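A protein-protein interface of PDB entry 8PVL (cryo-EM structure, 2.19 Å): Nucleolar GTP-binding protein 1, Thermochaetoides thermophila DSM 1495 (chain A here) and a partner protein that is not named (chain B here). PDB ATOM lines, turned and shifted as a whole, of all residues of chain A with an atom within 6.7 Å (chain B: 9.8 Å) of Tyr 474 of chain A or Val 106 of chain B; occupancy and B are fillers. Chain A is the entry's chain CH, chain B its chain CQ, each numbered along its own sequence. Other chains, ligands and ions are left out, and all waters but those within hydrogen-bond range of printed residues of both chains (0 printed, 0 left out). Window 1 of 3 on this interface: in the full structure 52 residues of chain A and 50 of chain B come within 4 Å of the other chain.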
ATOM      1  N   GLU A 464      -5.253 -13.688  30.269  1.00  0.00           N
ATOM      2  CA  GLU A 464      -5.877 -12.962  29.166  1.00  0.00           C
ATOM      3  C   GLU A 464      -6.380 -13.918  28.090  1.00  0.00           C
ATOM      4  O   GLU A 464      -7.458 -13.711  27.521  1.00  0.00           O
ATOM      5  CB  GLU A 464      -4.883 -11.963  28.575  1.00  0.00           C
ATOM      6  CG  GLU A 464      -5.418 -11.152  27.406  1.00  0.00           C
ATOM      7  CD  GLU A 464      -4.349 -10.295  26.758  1.00  0.00           C
ATOM      8  OE1 GLU A 464      -3.167 -10.438  27.131  1.00  0.00           O
ATOM      9  OE2 GLU A 464      -4.691  -9.480  25.876  1.00  0.00           O
ATOM     10  N   GLU A 465      -5.612 -14.974  27.808  1.00  0.00           N
ATOM     11  CA  GLU A 465      -6.034 -15.973  26.830  1.00  0.00           C
ATOM     12  C   GLU A 465      -7.289 -16.706  27.286  1.00  0.00           C
ATOM     13  O   GLU A 465      -8.204 -16.938  26.485  1.00  0.00           O
ATOM     14  CB  GLU A 465      -4.895 -16.962  26.576  1.00  0.00           C
ATOM     15  CG  GLU A 465      -5.152 -17.964  25.457  1.00  0.00           C
ATOM     16  CD  GLU A 465      -4.892 -17.398  24.071  1.00  0.00           C
ATOM     17  OE1 GLU A 465      -4.554 -16.201  23.958  1.00  0.00           O
ATOM     18  OE2 GLU A 465      -5.018 -18.158  23.089  1.00  0.00           O
ATOM     19  N   GLU A 466      -7.353 -17.070  28.570  1.00  0.00           N
ATOM     20  CA  GLU A 466      -8.549 -17.722  29.102  1.00  0.00           C
ATOM     21  C   GLU A 466      -9.757 -16.794  29.053  1.00  0.00           C
ATOM     22  O   GLU A 466     -10.866 -17.227  28.715  1.00  0.00           O
ATOM     23  CB  GLU A 466      -8.302 -18.199  30.534  1.00  0.00           C
ATOM     24  CG  GLU A 466      -7.263 -19.301  30.660  1.00  0.00           C
ATOM     25  CD  GLU A 466      -7.587 -20.517  29.812  1.00  0.00           C
ATOM     26  OE1 GLU A 466      -8.758 -20.952  29.815  1.00  0.00           O
ATOM     27  OE2 GLU A 466      -6.670 -21.038  29.144  1.00  0.00           O
ATOM     28  N   LEU A 468     -10.247 -14.268  26.935  1.00  0.00           N
ATOM     29  CA  LEU A 468     -10.642 -14.129  25.535  1.00  0.00           C
ATOM     30  C   LEU A 468     -11.366 -15.373  25.033  1.00  0.00           C
ATOM     31  O   LEU A 468     -12.349 -15.268  24.286  1.00  0.00           O
ATOM     32  CB  LEU A 468      -9.414 -13.836  24.674  1.00  0.00           C
ATOM     33  CG  LEU A 468      -8.826 -12.427  24.771  1.00  0.00           C
ATOM     34  CD1 LEU A 468      -7.559 -12.316  23.939  1.00  0.00           C
ATOM     35  CD2 LEU A 468      -9.842 -11.382  24.344  1.00  0.00           C
ATOM     36  N   GLU A 469     -10.900 -16.560  25.434  1.00  0.00           N
ATOM     37  CA  GLU A 469     -11.554 -17.794  25.015  1.00  0.00           C
ATOM     38  C   GLU A 469     -12.943 -17.927  25.629  1.00  0.00           C
ATOM     39  O   GLU A 469     -13.857 -18.463  24.993  1.00  0.00           O
ATOM     40  CB  GLU A 469     -10.683 -18.996  25.380  1.00  0.00           C
ATOM     41  CG  GLU A 469     -10.719 -20.116  24.356  1.00  0.00           C
ATOM     42  CD  GLU A 469      -9.371 -20.785  24.182  1.00  0.00           C
ATOM     43  OE1 GLU A 469      -8.422 -20.407  24.898  1.00  0.00           O
ATOM     44  OE2 GLU A 469      -9.261 -21.689  23.326  1.00  0.00           O
ATOM     45  N   GLU A 471     -14.829 -15.255  26.433  1.00  0.00           N
ATOM     46  CA  GLU A 471     -15.629 -14.230  25.775  1.00  0.00           C
ATOM     47  C   GLU A 471     -15.897 -14.535  24.308  1.00  0.00           C
ATOM     48  O   GLU A 471     -16.727 -13.855  23.697  1.00  0.00           O
ATOM     49  CB  GLU A 471     -14.943 -12.868  25.892  1.00  0.00           C
ATOM     50  CG  GLU A 471     -14.975 -12.273  27.287  1.00  0.00           C
ATOM     51  CD  GLU A 471     -14.384 -10.878  27.335  1.00  0.00           C
ATOM     52  OE1 GLU A 471     -14.109 -10.311  26.258  1.00  0.00           O
ATOM     53  OE2 GLU A 471     -14.196 -10.350  28.452  1.00  0.00           O
ATOM     54  N   GLY A 472     -15.221 -15.521  23.730  1.00  0.00           N
ATOM     55  CA  GLY A 472     -15.456 -15.846  22.337  1.00  0.00           C
ATOM     56  C   GLY A 472     -14.676 -14.978  21.380  1.00  0.00           C
ATOM     57  O   GLY A 472     -15.232 -14.497  20.388  1.00  0.00           O
ATOM     58  N   PHE A 473     -13.399 -14.739  21.673  1.00  0.00           N
ATOM     59  CA  PHE A 473     -12.550 -13.951  20.791  1.00  0.00           C
ATOM     60  C   PHE A 473     -12.086 -14.756  19.585  1.00  0.00           C
ATOM     61  O   PHE A 473     -11.908 -14.192  18.500  1.00  0.00           O
ATOM     62  CB  PHE A 473     -11.355 -13.423  21.585  1.00  0.00           C
ATOM     63  CG  PHE A 473     -10.431 -12.541  20.800  1.00  0.00           C
ATOM     64  CD1 PHE A 473     -10.754 -11.216  20.565  1.00  0.00           C
ATOM     65  CD2 PHE A 473      -9.224 -13.028  20.325  1.00  0.00           C
ATOM     66  CE1 PHE A 473      -9.901 -10.397  19.854  1.00  0.00           C
ATOM     67  CE2 PHE A 473      -8.367 -12.214  19.613  1.00  0.00           C
ATOM     68  CZ  PHE A 473      -8.706 -10.896  19.378  1.00  0.00           C
ATOM     69  N   TYR A 474     -11.895 -16.063  19.750  1.00  0.00           N
ATOM     70  CA  TYR A 474     -11.332 -16.920  18.717  1.00  0.00           C
ATOM     71  C   TYR A 474     -12.381 -17.758  17.997  1.00  0.00           C
ATOM     72  O   TYR A 474     -12.017 -18.681  17.261  1.00  0.00           O
ATOM     73  CB  TYR A 474     -10.272 -17.845  19.319  1.00  0.00           C
ATOM     74  CG  TYR A 474      -9.126 -17.136  20.003  1.00  0.00           C
ATOM     75  CD1 TYR A 474      -8.021 -16.703  19.281  1.00  0.00           C
ATOM     76  CD2 TYR A 474      -9.140 -16.914  21.374  1.00  0.00           C
ATOM     77  CE1 TYR A 474      -6.968 -16.061  19.903  1.00  0.00           C
ATOM     78  CE2 TYR A 474      -8.093 -16.272  22.005  1.00  0.00           C
ATOM     79  CZ  TYR A 474      -7.010 -15.848  21.263  1.00  0.00           C
ATOM     80  OH  TYR A 474      -5.966 -15.210  21.890  1.00  0.00           O
ATOM     81  N   ASP A 475     -13.666 -17.472  18.195  1.00  0.00           N
ATOM     82  CA  ASP A 475     -14.707 -18.299  17.600  1.00  0.00           C
ATOM     83  C   ASP A 475     -14.806 -18.062  16.096  1.00  0.00           C
ATOM     84  O   ASP A 475     -14.454 -16.996  15.584  1.00  0.00           O
ATOM     85  CB  ASP A 475     -16.058 -18.029  18.268  1.00  0.00           C
ATOM     86  CG  ASP A 475     -16.451 -16.562  18.241  1.00  0.00           C
ATOM     87  OD1 ASP A 475     -15.619 -15.714  17.858  1.00  0.00           O
ATOM     88  OD2 ASP A 475     -17.605 -16.256  18.608  1.00  0.00           O
ATOM     89  N   GLU A 476     -15.284 -19.080  15.386  1.00  0.00           N
ATOM     90  CA  GLU A 476     -15.456 -19.020  13.944  1.00  0.00           C
ATOM     91  C   GLU A 476     -16.914 -19.275  13.588  1.00  0.00           C
ATOM     92  O   GLU A 476     -17.597 -20.076  14.234  1.00  0.00           O
ATOM     93  CB  GLU A 476     -14.557 -20.037  13.231  1.00  0.00           C
ATOM     94  CG  GLU A 476     -13.081 -19.900  13.565  1.00  0.00           C
ATOM     95  CD  GLU A 476     -12.213 -20.869  12.788  1.00  0.00           C
ATOM     96  OE1 GLU A 476     -12.759 -21.619  11.951  1.00  0.00           O
ATOM     97  OE2 GLU A 476     -10.984 -20.880  13.011  1.00  0.00           O
ATOM     98  N   MET B  63      -0.595  -6.348  13.065  1.00  0.00           N
ATOM     99  CA  MET B  63      -1.002  -6.341  14.463  1.00  0.00           C
ATOM    100  C   MET B  63       0.104  -5.715  15.304  1.00  0.00           C
ATOM    101  O   MET B  63       1.228  -6.223  15.337  1.00  0.00           O
ATOM    102  CB  MET B  63      -1.299  -7.763  14.926  1.00  0.00           C
ATOM    103  CG  MET B  63      -2.336  -7.866  16.021  1.00  0.00           C
ATOM    104  SD  MET B  63      -2.520  -9.563  16.592  1.00  0.00           S
ATOM    105  CE  MET B  63      -0.817  -9.989  16.943  1.00  0.00           C
ATOM    106  N   ASP B  66      -0.842  -5.424  20.976  1.00  0.00           N
ATOM    107  CA  ASP B  66      -1.058  -6.792  21.424  1.00  0.00           C
ATOM    108  C   ASP B  66      -0.101  -7.072  22.571  1.00  0.00           C
ATOM    109  O   ASP B  66       1.025  -6.570  22.592  1.00  0.00           O
ATOM    110  CB  ASP B  66      -0.847  -7.802  20.290  1.00  0.00           C
ATOM    111  CG  ASP B  66      -1.650  -9.071  20.484  1.00  0.00           C
ATOM    112  OD1 ASP B  66      -2.883  -9.031  20.288  1.00  0.00           O
ATOM    113  OD2 ASP B  66      -1.052 -10.111  20.829  1.00  0.00           O
ATOM    114  N   SER B  67      -0.564  -7.879  23.525  1.00  0.00           N
ATOM    115  CA  SER B  67       0.254  -8.175  24.696  1.00  0.00           C
ATOM    116  C   SER B  67       1.405  -9.116  24.362  1.00  0.00           C
ATOM    117  O   SER B  67       2.421  -9.119  25.066  1.00  0.00           O
ATOM    118  CB  SER B  67      -0.616  -8.765  25.804  1.00  0.00           C
ATOM    119  OG  SER B  67      -0.548 -10.177  25.803  1.00  0.00           O
ATOM    120  N   THR B  68       1.274  -9.911  23.300  1.00  0.00           N
ATOM    121  CA  THR B  68       2.336 -10.829  22.908  1.00  0.00           C
ATOM    122  C   THR B  68       3.533 -10.125  22.284  1.00  0.00           C
ATOM    123  O   THR B  68       4.585 -10.753  22.130  1.00  0.00           O
ATOM    124  CB  THR B  68       1.800 -11.875  21.931  1.00  0.00           C
ATOM    125  OG1 THR B  68       1.290 -11.221  20.763  1.00  0.00           O
ATOM    126  CG2 THR B  68       0.698 -12.687  22.576  1.00  0.00           C
ATOM    127  N   ARG B  95       5.268 -20.700  23.682  1.00  0.00           N
ATOM    128  CA  ARG B  95       3.867 -20.398  23.978  1.00  0.00           C
ATOM    129  C   ARG B  95       3.448 -19.041  23.407  1.00  0.00           C
ATOM    130  O   ARG B  95       2.344 -18.899  22.853  1.00  0.00           O
ATOM    131  CB  ARG B  95       3.640 -20.441  25.489  1.00  0.00           C
ATOM    132  CG  ARG B  95       2.209 -20.191  25.917  1.00  0.00           C
ATOM    133  CD  ARG B  95       1.260 -21.185  25.273  1.00  0.00           C
ATOM    134  NE  ARG B  95      -0.108 -21.014  25.749  1.00  0.00           N
ATOM    135  CZ  ARG B  95      -1.186 -21.376  25.068  1.00  0.00           C
ATOM    136  NH1 ARG B  95      -1.092 -21.938  23.875  1.00  0.00           N
ATOM    137  NH2 ARG B  95      -2.387 -21.163  25.596  1.00  0.00           N
ATOM    138  N   ILE B  96       4.329 -18.043  23.519  1.00  0.00           N
ATOM    139  CA  ILE B  96       4.063 -16.707  22.996  1.00  0.00           C
ATOM    140  C   ILE B  96       3.924 -16.744  21.482  1.00  0.00           C
ATOM    141  O   ILE B  96       3.048 -16.079  20.912  1.00  0.00           O
ATOM    142  CB  ILE B  96       5.172 -15.734  23.449  1.00  0.00           C
ATOM    143  CG1 ILE B  96       4.986 -15.350  24.915  1.00  0.00           C
ATOM    144  CG2 ILE B  96       5.218 -14.476  22.591  1.00  0.00           C
ATOM    145  CD1 ILE B  96       6.268 -14.930  25.580  1.00  0.00           C
ATOM    146  N   GLU B  98       2.849 -19.280  19.638  1.00  0.00           N
ATOM    147  CA  GLU B  98       1.549 -19.872  19.300  1.00  0.00           C
ATOM    148  C   GLU B  98       0.401 -18.879  19.502  1.00  0.00           C
ATOM    149  O   GLU B  98      -0.479 -18.730  18.632  1.00  0.00           O
ATOM    150  CB  GLU B  98       1.318 -21.134  20.132  1.00  0.00           C
ATOM    151  CG  GLU B  98       2.345 -22.228  19.907  1.00  0.00           C
ATOM    152  CD  GLU B  98       2.314 -23.288  20.993  1.00  0.00           C
ATOM    153  OE1 GLU B  98       1.530 -23.134  21.954  1.00  0.00           O
ATOM    154  OE2 GLU B  98       3.073 -24.273  20.885  1.00  0.00           O
ATOM    155  N   ILE B  99       0.407 -18.175  20.641  1.00  0.00           N
ATOM    156  CA  ILE B  99      -0.667 -17.226  20.939  1.00  0.00           C
ATOM    157  C   ILE B  99      -0.659 -16.070  19.940  1.00  0.00           C
ATOM    158  O   ILE B  99      -1.719 -15.605  19.487  1.00  0.00           O
ATOM    159  CB  ILE B  99      -0.546 -16.735  22.394  1.00  0.00           C
ATOM    160  CG1 ILE B  99      -0.758 -17.901  23.362  1.00  0.00           C
ATOM    161  CG2 ILE B  99      -1.551 -15.639  22.691  1.00  0.00           C
ATOM    162  CD1 ILE B  99      -0.604 -17.526  24.814  1.00  0.00           C
ATOM    163  N   ARG B 100       0.538 -15.612  19.558  1.00  0.00           N
ATOM    164  CA  ARG B 100       0.662 -14.536  18.581  1.00  0.00           C
ATOM    165  C   ARG B 100       0.133 -14.957  17.216  1.00  0.00           C
ATOM    166  O   ARG B 100      -0.509 -14.158  16.523  1.00  0.00           O
ATOM    167  CB  ARG B 100       2.120 -14.094  18.479  1.00  0.00           C
ATOM    168  CG  ARG B 100       2.368 -12.974  17.487  1.00  0.00           C
ATOM    169  CD  ARG B 100       3.815 -12.527  17.510  1.00  0.00           C
ATOM    170  NE  ARG B 100       4.075 -11.493  16.517  1.00  0.00           N
ATOM    171  CZ  ARG B 100       5.201 -10.797  16.438  1.00  0.00           C
ATOM    172  NH1 ARG B 100       6.200 -10.999  17.282  1.00  0.00           N
ATOM    173  NH2 ARG B 100       5.327  -9.874  15.489  1.00  0.00           N
ATOM    174  N   ALA B 101       0.387 -16.208  16.813  1.00  0.00           N
ATOM    175  CA  ALA B 101      -0.151 -16.694  15.543  1.00  0.00           C
ATOM    176  C   ALA B 101      -1.678 -16.701  15.545  1.00  0.00           C
ATOM    177  O   ALA B 101      -2.313 -16.265  14.567  1.00  0.00           O
ATOM    178  CB  ALA B 101       0.392 -18.090  15.244  1.00  0.00           C
ATOM    179  N   ARG B 102      -2.285 -17.167  16.646  1.00  0.00           N
ATOM    180  CA  ARG B 102      -3.748 -17.178  16.733  1.00  0.00           C
ATOM    181  C   ARG B 102      -4.328 -15.764  16.663  1.00  0.00           C
ATOM    182  O   ARG B 102      -5.292 -15.501  15.920  1.00  0.00           O
ATOM    183  CB  ARG B 102      -4.194 -17.870  18.022  1.00  0.00           C
ATOM    184  CG  ARG B 102      -3.909 -19.356  18.069  1.00  0.00           C
ATOM    185  CD  ARG B 102      -4.461 -19.980  19.341  1.00  0.00           C
ATOM    186  NE  ARG B 102      -5.889 -20.265  19.242  1.00  0.00           N
ATOM    187  CZ  ARG B 102      -6.776 -19.985  20.187  1.00  0.00           C
ATOM    188  NH1 ARG B 102      -6.422 -19.395  21.317  1.00  0.00           N
ATOM    189  NH2 ARG B 102      -8.051 -20.307  19.995  1.00  0.00           N
ATOM    190  N   ARG B 103      -3.732 -14.830  17.410  1.00  0.00           N
ATOM    191  CA  ARG B 103      -4.253 -13.466  17.421  1.00  0.00           C
ATOM    192  C   ARG B 103      -4.033 -12.759  16.087  1.00  0.00           C
ATOM    193  O   ARG B 103      -4.863 -11.934  15.683  1.00  0.00           O
ATOM    194  CB  ARG B 103      -3.625 -12.678  18.568  1.00  0.00           C
ATOM    195  CG  ARG B 103      -4.062 -13.179  19.931  1.00  0.00           C
ATOM    196  CD  ARG B 103      -3.597 -12.270  21.048  1.00  0.00           C
ATOM    197  NE  ARG B 103      -3.968 -12.798  22.355  1.00  0.00           N
ATOM    198  CZ  ARG B 103      -3.585 -12.273  23.510  1.00  0.00           C
ATOM    199  NH1 ARG B 103      -2.818 -11.198  23.559  1.00  0.00           N
ATOM    200  NH2 ARG B 103      -3.981 -12.844  24.644  1.00  0.00           N
ATOM    201  N   GLU B 104      -2.948 -13.084  15.379  1.00  0.00           N
ATOM    202  CA  GLU B 104      -2.733 -12.519  14.052  1.00  0.00           C
ATOM    203  C   GLU B 104      -3.782 -13.010  13.063  1.00  0.00           C
ATOM    204  O   GLU B 104      -4.248 -12.238  12.213  1.00  0.00           O
ATOM    205  CB  GLU B 104      -1.328 -12.861  13.555  1.00  0.00           C
ATOM    206  CG  GLU B 104      -0.819 -11.944  12.453  1.00  0.00           C
ATOM    207  CD  GLU B 104      -1.254 -12.392  11.070  1.00  0.00           C
ATOM    208  OE1 GLU B 104      -1.266 -13.615  10.816  1.00  0.00           O
ATOM    209  OE2 GLU B 104      -1.595 -11.523  10.241  1.00  0.00           O
ATOM    210  N   ARG B 105      -4.151 -14.294  13.145  1.00  0.00           N
ATOM    211  CA  ARG B 105      -5.208 -14.800  12.270  1.00  0.00           C
ATOM    212  C   ARG B 105      -6.539 -14.107  12.550  1.00  0.00           C
ATOM    213  O   ARG B 105      -7.282 -13.763  11.615  1.00  0.00           O
ATOM    214  CB  ARG B 105      -5.339 -16.316  12.421  1.00  0.00           C
ATOM    215  CG  ARG B 105      -6.501 -16.912  11.647  1.00  0.00           C
ATOM    216  CD  ARG B 105      -6.356 -18.410  11.490  1.00  0.00           C
ATOM    217  NE  ARG B 105      -5.627 -18.755  10.276  1.00  0.00           N
ATOM    218  CZ  ARG B 105      -6.196 -19.169   9.152  1.00  0.00           C
ATOM    219  NH1 ARG B 105      -7.507 -19.302   9.049  1.00  0.00           N
ATOM    220  NH2 ARG B 105      -5.428 -19.458   8.106  1.00  0.00           N
ATOM    221  N   VAL B 106      -6.842 -13.870  13.832  1.00  0.00           N
ATOM    222  CA  VAL B 106      -8.066 -13.142  14.185  1.00  0.00           C
ATOM    223  C   VAL B 106      -8.034 -11.718  13.627  1.00  0.00           C
ATOM    224  O   VAL B 106      -9.036 -11.219  13.092  1.00  0.00           O
ATOM    225  CB  VAL B 106      -8.271 -13.154  15.711  1.00  0.00           C
ATOM    226  CG1 VAL B 106      -9.427 -12.251  16.111  1.00  0.00           C
ATOM    227  CG2 VAL B 106      -8.513 -14.571  16.196  1.00  0.00           C
ATOM    228  N   PHE B 107      -6.877 -11.054  13.731  1.00  0.00           N
ATOM    229  CA  PHE B 107      -6.711  -9.702  13.194  1.00  0.00           C
ATOM    230  C   PHE B 107      -6.937  -9.661  11.684  1.00  0.00           C
ATOM    231  O   PHE B 107      -7.622  -8.762  11.171  1.00  0.00           O
ATOM    232  CB  PHE B 107      -5.307  -9.199  13.549  1.00  0.00           C
ATOM    233  CG  PHE B 107      -5.018  -7.789  13.113  1.00  0.00           C
ATOM    234  CD1 PHE B 107      -5.379  -6.717  13.910  1.00  0.00           C
ATOM    235  CD2 PHE B 107      -4.341  -7.537  11.927  1.00  0.00           C
ATOM    236  CE1 PHE B 107      -5.099  -5.421  13.521  1.00  0.00           C
ATOM    237  CE2 PHE B 107      -4.062  -6.244  11.532  1.00  0.00           C
ATOM    238  CZ  PHE B 107      -4.440  -5.184  12.331  1.00  0.00           C
ATOM    239  N   TYR B 108      -6.386 -10.639  10.960  1.00  0.00           N
ATOM    240  CA  TYR B 108      -6.552 -10.667   9.509  1.00  0.00           C
ATOM    241  C   TYR B 108      -8.005 -10.917   9.110  1.00  0.00           C
ATOM    242  O   TYR B 108      -8.502 -10.313   8.149  1.00  0.00           O
ATOM    243  CB  TYR B 108      -5.641 -11.723   8.890  1.00  0.00           C
ATOM    244  CG  TYR B 108      -5.633 -11.695   7.380  1.00  0.00           C
ATOM    245  CD1 TYR B 108      -4.915 -10.729   6.689  1.00  0.00           C
ATOM    246  CD2 TYR B 108      -6.355 -12.625   6.646  1.00  0.00           C
ATOM    247  CE1 TYR B 108      -4.908 -10.698   5.309  1.00  0.00           C
ATOM    248  CE2 TYR B 108      -6.354 -12.601   5.267  1.00  0.00           C
ATOM    249  CZ  TYR B 108      -5.631 -11.636   4.604  1.00  0.00           C
ATOM    250  OH  TYR B 108      -5.631 -11.612   3.230  1.00  0.00           O
ATOM    251  N   LYS B 109      -8.700 -11.807   9.825  1.00  0.00           N
ATOM    252  CA  LYS B 109     -10.107 -12.053   9.505  1.00  0.00           C
ATOM    253  C   LYS B 109     -10.967 -10.824   9.791  1.00  0.00           C
ATOM    254  O   LYS B 109     -11.913 -10.526   9.041  1.00  0.00           O
ATOM    255  CB  LYS B 109     -10.616 -13.267  10.277  1.00  0.00           C
ATOM    256  CG  LYS B 109     -10.050 -14.580   9.774  1.00  0.00           C
ATOM    257  CD  LYS B 109     -10.661 -15.763  10.500  1.00  0.00           C
ATOM    258  CE  LYS B 109     -11.723 -16.436   9.649  1.00  0.00           C
ATOM    259  NZ  LYS B 109     -12.941 -16.762  10.440  1.00  0.00           N
ATOM    260  N   LYS B 110     -10.649 -10.096  10.867  1.00  0.00           N
ATOM    261  CA  LYS B 110     -11.338  -8.837  11.131  1.00  0.00           C
ATOM    262  C   LYS B 110     -11.077  -7.814  10.034  1.00  0.00           C
ATOM    263  O   LYS B 110     -11.953  -6.996   9.732  1.00  0.00           O
ATOM    264  CB  LYS B 110     -10.917  -8.277  12.489  1.00  0.00           C
ATOM    265  CG  LYS B 110     -11.816  -8.704  13.634  1.00  0.00           C
ATOM    266  CD  LYS B 110     -11.655  -7.787  14.832  1.00  0.00           C
ATOM    267  CE  LYS B 110     -11.317  -8.576  16.085  1.00  0.00           C
ATOM    268  NZ  LYS B 110     -12.211  -9.754  16.253  1.00  0.00           N
ATOM    269  N   ARG B 111      -9.881  -7.833   9.438  1.00  0.00           N
ATOM    270  CA  ARG B 111      -9.640  -6.988   8.270  1.00  0.00           C
ATOM    271  C   ARG B 111     -10.489  -7.416   7.073  1.00  0.00           C
ATOM    272  O   ARG B 111     -11.024  -6.567   6.351  1.00  0.00           O
ATOM    273  CB  ARG B 111      -8.158  -6.996   7.892  1.00  0.00           C
ATOM    274  CG  ARG B 111      -7.265  -6.202   8.822  1.00  0.00           C
ATOM    275  CD  ARG B 111      -6.150  -5.503   8.059  1.00  0.00           C
ATOM    276  NE  ARG B 111      -5.195  -6.439   7.479  1.00  0.00           N
ATOM    277  CZ  ARG B 111      -4.821  -6.438   6.208  1.00  0.00           C
ATOM    278  NH1 ARG B 111      -5.306  -5.562   5.344  1.00  0.00           N
ATOM    279  NH2 ARG B 111      -3.931  -7.335   5.793  1.00  0.00           N
ATOM    280  N   MET B 112     -10.625  -8.725   6.844  1.00  0.00           N
ATOM    281  CA  MET B 112     -11.242  -9.239   5.623  1.00  0.00           C
ATOM    282  C   MET B 112     -12.707  -9.647   5.803  1.00  0.00           C
ATOM    283  O   MET B 112     -13.195 -10.498   5.049  1.00  0.00           O
ATOM    284  CB  MET B 112     -10.437 -10.424   5.088  1.00  0.00           C
ATOM    285  CG  MET B 112      -8.990 -10.100   4.762  1.00  0.00           C
ATOM    286  SD  MET B 112      -8.820  -9.031   3.322  1.00  0.00           S
ATOM    287  CE  MET B 112      -7.423  -8.028   3.813  1.00  0.00           C
ATOM    288  N   ALA B 113     -13.389  -9.100   6.814  1.00  0.00           N
ATOM    289  CA  ALA B 113     -14.811  -9.373   7.058  1.00  0.00           C
ATOM    290  C   ALA B 113     -15.720  -9.193   5.828  1.00  0.00           C
ATOM    291  O   ALA B 113     -16.337 -10.157   5.362  1.00  0.00           O
ATOM    292  CB  ALA B 113     -15.302  -8.487   8.205  1.00  0.00           C
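The guanidinium group (NH2) of Arg 102 of chain B lies within salt-bridge range of the side-chain carboxylate (OE2) of Glu 469 of chain A (3.8 Å). NH1 of Arg 102 of chain B lies within salt-bridge range of OE2 of Glu 465 of chain A (2.6 Å). NH1 of Arg 103 of chain B is in salt-bridge range of OE2 of Glu 464 of chain A (3.4 Å). The side-chain hydroxyl of Ser 67 of chain B lies within hydrogen-bond range of the side-chain carboxylate of Glu 464 of chain A, 2.9 Å away. OE1 of Glu 465 of chain A is in salt-bridge range of NH2 of Arg 103 of chain B, at 3.5 Å. The guanidinium group (NE) of Arg 103 of chain B lies within hydrogen-bond range of the side-chain hydroxyl (OH) of Tyr 474 of chain A.
N of Phe 473 of chain A lies within hydrogen-bond range of O of Leu 468 of chain A. The guanidinium group (NH1) of Arg 103 of chain B lies within salt-bridge range of the side-chain carboxylate (OD2) of Asp 66 of chain B (3.4 Å). The side-chain hydroxyl of Ser 67 of chain B is in hydrogen-bond range of the guanidinium group of Arg 103 of chain B (3.4 Å). The side-chain carboxylate of Glu 465 of chain A is in hydrogen-bond range of the side-chain hydroxyl of Tyr 474 of chain A.
OE1 of Glu 465 of chain A touches CG2 of Ile 99 of chain B (3.3 Å). NH2 of Arg 103 of chain B touches CD1 of Leu 468 of chain A (3.7 Å). Phe 473 of chain A touches Val 106 of chain B. Tyr 474 of chain A touches Arg 102 of chain B. Tyr 474 of chain A touches Val 106 of chain B.
Of chain B, only Arg 102 (3.3 Å), Arg 103 (3.2 Å) and Val 106 (3.8 Å) come within 4 Å of Tyr 474 of chain A. Of chain A, only Phe 473 and Tyr 474 come within 4 Å of Val 106 of chain B. Of chain B, only Arg 103 comes within 4 Å of Leu 468 of chain A. No residue of chain B comes within 4 Å of Asp 475 of chain A. Of the printed residues of chain B, Glu 469 of chain A touches Arg 102. Of the printed residues of chain B, Glu 464 of chain A touches Ser 67 (2.9 Å) and Arg 103 (3.3 Å). Arg 95 of chain B touches none of the printed residues of chain A. Glu 466 of chain A touches none of the printed residues of chain B. The nearest residue of chain B that does not touch Tyr 474 of chain A is Ile 99 of chain B (4.5 Å). The nearest residue of chain A that does not touch Val 106 of chain B is Asp 475 of chain A (6.2 Å).
Printed residues of chain A that touch a printed residue of chain B: Glu 464, Glu 465, Leu 468, Glu 469, Phe 473 and Tyr 474. Hydrophobic or aromatic side chains of chain B that line the printed part of chain A: Ile 99 and Val 106.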
